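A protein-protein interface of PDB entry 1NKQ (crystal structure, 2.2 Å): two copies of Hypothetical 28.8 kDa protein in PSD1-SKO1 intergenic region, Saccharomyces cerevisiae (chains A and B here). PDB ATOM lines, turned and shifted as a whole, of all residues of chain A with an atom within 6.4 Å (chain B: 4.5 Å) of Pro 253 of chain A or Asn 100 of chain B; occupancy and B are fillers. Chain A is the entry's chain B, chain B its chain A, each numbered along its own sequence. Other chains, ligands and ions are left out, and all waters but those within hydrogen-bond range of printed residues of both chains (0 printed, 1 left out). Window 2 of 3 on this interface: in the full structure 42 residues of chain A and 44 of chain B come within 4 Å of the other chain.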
ATOM      1  N   ASN A  60     -10.484 -17.443  19.526  1.00  0.00           N
ATOM      2  CA  ASN A  60     -10.198 -18.628  20.328  1.00  0.00           C
ATOM      3  C   ASN A  60      -9.236 -19.607  19.633  1.00  0.00           C
ATOM      4  O   ASN A  60      -9.062 -20.736  20.080  1.00  0.00           O
ATOM      5  CB  ASN A  60     -11.520 -19.327  20.668  1.00  0.00           C
ATOM      6  CG  ASN A  60     -11.491 -20.029  22.017  1.00  0.00           C
ATOM      7  OD1 ASN A  60     -11.336 -19.390  23.062  1.00  0.00           O
ATOM      8  ND2 ASN A  60     -11.650 -21.354  22.000  1.00  0.00           N
ATOM      9  N   SER A  61      -8.611 -19.162  18.545  1.00  0.00           N
ATOM     10  CA  SER A  61      -7.660 -19.980  17.791  1.00  0.00           C
ATOM     11  C   SER A  61      -6.246 -19.843  18.357  1.00  0.00           C
ATOM     12  O   SER A  61      -5.791 -18.739  18.653  1.00  0.00           O
ATOM     13  CB  SER A  61      -7.651 -19.555  16.324  1.00  0.00           C
ATOM     14  OG  SER A  61      -6.534 -20.090  15.636  1.00  0.00           O
ATOM     15  N   THR A  62      -5.545 -20.962  18.505  1.00  0.00           N
ATOM     16  CA  THR A  62      -4.192 -20.918  19.037  1.00  0.00           C
ATOM     17  C   THR A  62      -3.181 -21.248  17.956  1.00  0.00           C
ATOM     18  O   THR A  62      -1.997 -21.411  18.215  1.00  0.00           O
ATOM     19  CB  THR A  62      -4.031 -21.859  20.258  1.00  0.00           C
ATOM     20  OG1 THR A  62      -4.697 -23.102  20.003  1.00  0.00           O
ATOM     21  CG2 THR A  62      -4.629 -21.207  21.515  1.00  0.00           C
ATOM     22  N   PHE A  63      -3.679 -21.355  16.733  1.00  0.00           N
ATOM     23  CA  PHE A  63      -2.858 -21.600  15.556  1.00  0.00           C
ATOM     24  C   PHE A  63      -3.775 -21.616  14.348  1.00  0.00           C
ATOM     25  O   PHE A  63      -4.720 -22.408  14.281  1.00  0.00           O
ATOM     26  CB  PHE A  63      -2.088 -22.918  15.626  1.00  0.00           C
ATOM     27  CG  PHE A  63      -1.211 -23.141  14.426  1.00  0.00           C
ATOM     28  CD1 PHE A  63      -0.087 -22.344  14.220  1.00  0.00           C
ATOM     29  CD2 PHE A  63      -1.541 -24.096  13.467  1.00  0.00           C
ATOM     30  CE1 PHE A  63       0.692 -22.489  13.078  1.00  0.00           C
ATOM     31  CE2 PHE A  63      -0.768 -24.250  12.321  1.00  0.00           C
ATOM     32  CZ  PHE A  63       0.352 -23.445  12.125  1.00  0.00           C
ATOM     33  N   ASP A 145       0.116 -26.533  20.468  1.00  0.00           N
ATOM     34  CA  ASP A 145       0.384 -25.334  19.691  1.00  0.00           C
ATOM     35  C   ASP A 145       1.374 -24.461  20.459  1.00  0.00           C
ATOM     36  O   ASP A 145       1.362 -24.418  21.690  1.00  0.00           O
ATOM     37  CB  ASP A 145      -0.898 -24.542  19.428  1.00  0.00           C
ATOM     38  CG  ASP A 145      -1.957 -25.361  18.715  1.00  0.00           C
ATOM     39  OD1 ASP A 145      -1.599 -26.242  17.905  1.00  0.00           O
ATOM     40  OD2 ASP A 145      -3.151 -25.113  18.956  1.00  0.00           O
ATOM     41  N   ARG A 250      -3.563 -20.879  27.644  1.00  0.00           N
ATOM     42  CA  ARG A 250      -4.171 -21.341  26.410  1.00  0.00           C
ATOM     43  C   ARG A 250      -5.665 -21.392  26.661  1.00  0.00           C
ATOM     44  O   ARG A 250      -6.108 -21.941  27.662  1.00  0.00           O
ATOM     45  CB  ARG A 250      -3.720 -22.752  26.031  1.00  0.00           C
ATOM     46  CG  ARG A 250      -4.398 -23.248  24.742  1.00  0.00           C
ATOM     47  CD  ARG A 250      -4.241 -24.752  24.526  1.00  0.00           C
ATOM     48  NE  ARG A 250      -4.903 -25.205  23.298  1.00  0.00           N
ATOM     49  CZ  ARG A 250      -4.265 -25.723  22.251  1.00  0.00           C
ATOM     50  NH1 ARG A 250      -2.946 -25.855  22.276  1.00  0.00           N
ATOM     51  NH2 ARG A 250      -4.943 -26.119  21.179  1.00  0.00           N
ATOM     52  N   PRO A 251      -6.462 -20.816  25.761  1.00  0.00           N
ATOM     53  CA  PRO A 251      -7.910 -20.850  25.959  1.00  0.00           C
ATOM     54  C   PRO A 251      -8.467 -22.245  25.679  1.00  0.00           C
ATOM     55  O   PRO A 251      -7.943 -23.247  26.171  1.00  0.00           O
ATOM     56  CB  PRO A 251      -8.413 -19.810  24.964  1.00  0.00           C
ATOM     57  CG  PRO A 251      -7.421 -19.917  23.854  1.00  0.00           C
ATOM     58  CD  PRO A 251      -6.103 -20.008  24.585  1.00  0.00           C
ATOM     59  N   GLY A 252      -9.533 -22.300  24.886  1.00  0.00           N
ATOM     60  CA  GLY A 252     -10.144 -23.569  24.533  1.00  0.00           C
ATOM     61  C   GLY A 252     -10.566 -24.380  25.741  1.00  0.00           C
ATOM     62  O   GLY A 252     -10.410 -23.925  26.878  1.00  0.00           O
ATOM     63  N   PRO A 253     -11.108 -25.592  25.522  1.00  0.00           N
ATOM     64  CA  PRO A 253     -11.562 -26.480  26.595  1.00  0.00           C
ATOM     65  C   PRO A 253     -10.537 -27.479  27.132  1.00  0.00           C
ATOM     66  O   PRO A 253     -10.855 -28.260  28.028  1.00  0.00           O
ATOM     67  CB  PRO A 253     -12.741 -27.192  25.958  1.00  0.00           C
ATOM     68  CG  PRO A 253     -12.247 -27.395  24.558  1.00  0.00           C
ATOM     69  CD  PRO A 253     -11.632 -26.045  24.219  1.00  0.00           C
ATOM     70  N   TYR A 254      -9.317 -27.475  26.604  1.00  0.00           N
ATOM     71  CA  TYR A 254      -8.335 -28.438  27.095  1.00  0.00           C
ATOM     72  C   TYR A 254      -7.933 -28.213  28.539  1.00  0.00           C
ATOM     73  O   TYR A 254      -7.784 -27.079  28.990  1.00  0.00           O
ATOM     74  CB  TYR A 254      -7.058 -28.451  26.250  1.00  0.00           C
ATOM     75  CG  TYR A 254      -6.080 -29.506  26.743  1.00  0.00           C
ATOM     76  CD1 TYR A 254      -6.218 -30.844  26.370  1.00  0.00           C
ATOM     77  CD2 TYR A 254      -5.061 -29.178  27.645  1.00  0.00           C
ATOM     78  CE1 TYR A 254      -5.373 -31.832  26.886  1.00  0.00           C
ATOM     79  CE2 TYR A 254      -4.218 -30.153  28.167  1.00  0.00           C
ATOM     80  CZ  TYR A 254      -4.377 -31.478  27.786  1.00  0.00           C
ATOM     81  OH  TYR A 254      -3.560 -32.448  28.323  1.00  0.00           O
ATOM     82  N   GLU A 255      -7.746 -29.321  29.250  1.00  0.00           N
ATOM     83  CA  GLU A 255      -7.327 -29.312  30.644  1.00  0.00           C
ATOM     84  C   GLU A 255      -6.675 -30.643  30.993  1.00  0.00           C
ATOM     85  O   GLU A 255      -7.308 -31.699  30.887  1.00  0.00           O
ATOM     86  CB  GLU A 255      -8.512 -29.092  31.584  1.00  0.00           C
ATOM     87  CG  GLU A 255      -8.136 -29.268  33.066  1.00  0.00           C
ATOM     88  CD  GLU A 255      -9.329 -29.266  34.007  1.00  0.00           C
ATOM     89  OE1 GLU A 255      -9.174 -29.740  35.153  1.00  0.00           O
ATOM     90  OE2 GLU A 255     -10.411 -28.784  33.611  1.00  0.00           O
ATOM     91  N   LEU B  98      -9.275 -26.055  12.388  1.00  0.00           N
ATOM     92  CA  LEU B  98      -9.985 -26.482  13.580  1.00  0.00           C
ATOM     93  C   LEU B  98      -9.061 -26.254  14.758  1.00  0.00           C
ATOM     94  O   LEU B  98      -8.042 -26.920  14.899  1.00  0.00           O
ATOM     95  CB  LEU B  98     -10.359 -27.958  13.464  1.00  0.00           C
ATOM     96  CG  LEU B  98     -11.217 -28.263  12.227  1.00  0.00           C
ATOM     97  CD1 LEU B  98     -11.425 -29.770  12.083  1.00  0.00           C
ATOM     98  CD2 LEU B  98     -12.552 -27.528  12.339  1.00  0.00           C
ATOM     99  N   SER B  99      -9.415 -25.294  15.599  1.00  0.00           N
ATOM    100  CA  SER B  99      -8.589 -24.967  16.750  1.00  0.00           C
ATOM    101  C   SER B  99      -9.437 -24.692  17.976  1.00  0.00           C
ATOM    102  O   SER B  99     -10.265 -23.788  17.983  1.00  0.00           O
ATOM    103  CB  SER B  99      -7.715 -23.749  16.429  1.00  0.00           C
ATOM    104  OG  SER B  99      -6.917 -23.371  17.537  1.00  0.00           O
ATOM    105  N   ASN B 100      -9.227 -25.487  19.015  1.00  0.00           N
ATOM    106  CA  ASN B 100      -9.970 -25.326  20.246  1.00  0.00           C
ATOM    107  C   ASN B 100     -11.495 -25.401  20.049  1.00  0.00           C
ATOM    108  O   ASN B 100     -12.242 -24.597  20.604  1.00  0.00           O
ATOM    109  CB  ASN B 100      -9.569 -24.004  20.906  1.00  0.00           C
ATOM    110  CG  ASN B 100      -8.076 -23.933  21.203  1.00  0.00           C
ATOM    111  OD1 ASN B 100      -7.504 -24.863  21.772  1.00  0.00           O
ATOM    112  ND2 ASN B 100      -7.441 -22.826  20.825  1.00  0.00           N
ATOM    113  N   VAL B 101     -11.950 -26.368  19.252  1.00  0.00           N
ATOM    114  CA  VAL B 101     -13.385 -26.564  19.017  1.00  0.00           C
ATOM    115  C   VAL B 101     -14.011 -27.128  20.303  1.00  0.00           C
ATOM    116  O   VAL B 101     -13.500 -28.077  20.888  1.00  0.00           O
ATOM    117  CB  VAL B 101     -13.639 -27.561  17.850  1.00  0.00           C
ATOM    118  CG1 VAL B 101     -15.117 -27.904  17.767  1.00  0.00           C
ATOM    119  CG2 VAL B 101     -13.175 -26.953  16.528  1.00  0.00           C
ATOM    120  N   THR B 102     -15.116 -26.544  20.742  1.00  0.00           N
ATOM    121  CA  THR B 102     -15.771 -26.998  21.963  1.00  0.00           C
ATOM    122  C   THR B 102     -16.680 -28.204  21.766  1.00  0.00           C
ATOM    123  O   THR B 102     -16.812 -29.040  22.654  1.00  0.00           O
ATOM    124  CB  THR B 102     -16.584 -25.860  22.591  1.00  0.00           C
ATOM    125  OG1 THR B 102     -17.408 -25.253  21.583  1.00  0.00           O
ATOM    126  CG2 THR B 102     -15.655 -24.820  23.196  1.00  0.00           C
ATOM    127  N   SER B 201      -8.283 -30.967  18.062  1.00  0.00           N
ATOM    128  CA  SER B 201      -8.168 -29.521  17.889  1.00  0.00           C
ATOM    129  C   SER B 201      -7.894 -28.744  19.170  1.00  0.00           C
ATOM    130  O   SER B 201      -7.453 -27.602  19.105  1.00  0.00           O
ATOM    131  CB  SER B 201      -9.442 -28.954  17.269  1.00  0.00           C
ATOM    132  OG  SER B 201     -10.406 -28.729  18.283  1.00  0.00           O
ATOM    133  N   THR B 202      -8.152 -29.347  20.327  1.00  0.00           N
ATOM    134  CA  THR B 202      -7.941 -28.645  21.589  1.00  0.00           C
ATOM    135  C   THR B 202      -6.512 -28.714  22.127  1.00  0.00           C
ATOM    136  O   THR B 202      -6.201 -28.105  23.153  1.00  0.00           O
ATOM    137  CB  THR B 202      -8.914 -29.155  22.679  1.00  0.00           C
ATOM    138  OG1 THR B 202      -8.616 -30.519  23.000  1.00  0.00           O
ATOM    139  CG2 THR B 202     -10.349 -29.053  22.188  1.00  0.00           C
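Pro 253 of chain A touches just these residues of chain B: Asn 100, Val 101 and Thr 202. Asn 100 of chain B touches five residues of chain A. Printed residues of chain A within 4 Å of Val 101 of chain B: Pro 253 (3.9 Å). Of the printed residues of chain A, Thr 202 of chain B touches Arg 250, Pro 253 and Tyr 254. Of the printed residues of chain B, Ser 61 of chain A touches Ser 99 (3.5 Å). Asp 145 of chain A touches none of the printed residues of chain B.
No position is printed for both chains. Of the 14 pairs that touch across the chains among the printed residues, none has its exchanged pair printed and touching as well.
Among the printed residues, pairs that only touch across the chains: Asn 60 of chain A with Ser 99 of chain B (3.9 Å), Ser 61 of chain A with Ser 99 of chain B (3.5 Å), Phe 63 of chain A with Ser 99 of chain B (3.9 Å), Arg 250 of chain A with Ser 201 of chain B (3.6 Å), Gly 252 of chain A with Asn 100 of chain B (3.7 Å), Pro 253 of chain A with Asn 100 of chain B (3.9 Å), Pro 253 of chain A with Val 101 of chain B (3.9 Å), Pro 253 of chain A with Thr 202 of chain B (3.5 Å) and Tyr 254 of chain A with Thr 202 of chain B (3.2 Å).
Printed residues of chain B that touch a printed residue of chain A: Ser 99, Asn 100, Val 101, Ser 201 and Thr 202. Printed residues of chain A that touch a printed residue of chain B: Asn 60, Ser 61, Thr 62, Phe 63, Arg 250, Gly 252, Pro 253 and Tyr 254. Hydrophobic or aromatic side chains of chain A within 4 Å of the printed part of chain B: Pro 253 and Tyr 254. Among the printed residues, 14 pairs touch across the chains.
N of Thr 62 of chain A is in hydrogen-bond range of OG of Ser 99 of chain B (2.9 Å). The side-chain amide nitrogen (ND2) of Asn 100 of chain B lies within hydrogen-bond range of the backbone carbonyl oxygen (O) of Asn 60 of chain A, at 2.7 Å. The side-chain amide nitrogen (ND2) of Asn 100 of chain B sits at hydrogen-bond distance from the side-chain hydroxyl (OG1) of Thr 62 of chain A (2.9 Å). The guanidinium group (NH2) of Arg 250 of chain A lies within hydrogen-bond range of the side-chain amide oxygen (OD1) of Asn 100 of chain B, at 2.9 Å. O of Thr 202 of chain B lies within hydrogen-bond range of NH2 of Arg 250 of chain A.
The side-chain amide nitrogen (ND2) of Asn 100 of chain B sits at hydrogen-bond distance from the side-chain hydroxyl (OG) of Ser 99 of chain B, at 3.4 Å. The side-chain hydroxyl (OG) of Ser 201 of chain B lies within hydrogen-bond range of the backbone NH (N) of Val 101 of chain B (3.0 Å). The side-chain hydroxyl of Ser 61 of chain A sits at hydrogen-bond distance from the backbone carbonyl oxygen of Phe 63 of chain A (3.2 Å). The side-chain carboxylate of Asp 145 of chain A is in hydrogen-bond range of the side-chain hydroxyl of Thr 62 of chain A (2.7 Å). OG1 of Thr 62 of chain A lies within hydrogen-bond range of NH2 of Arg 250 of chain A, at 3.2 Å. NH2 of Arg 250 of chain A is in salt-bridge range of OD2 of Asp 145 of chain A (3.0 Å).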
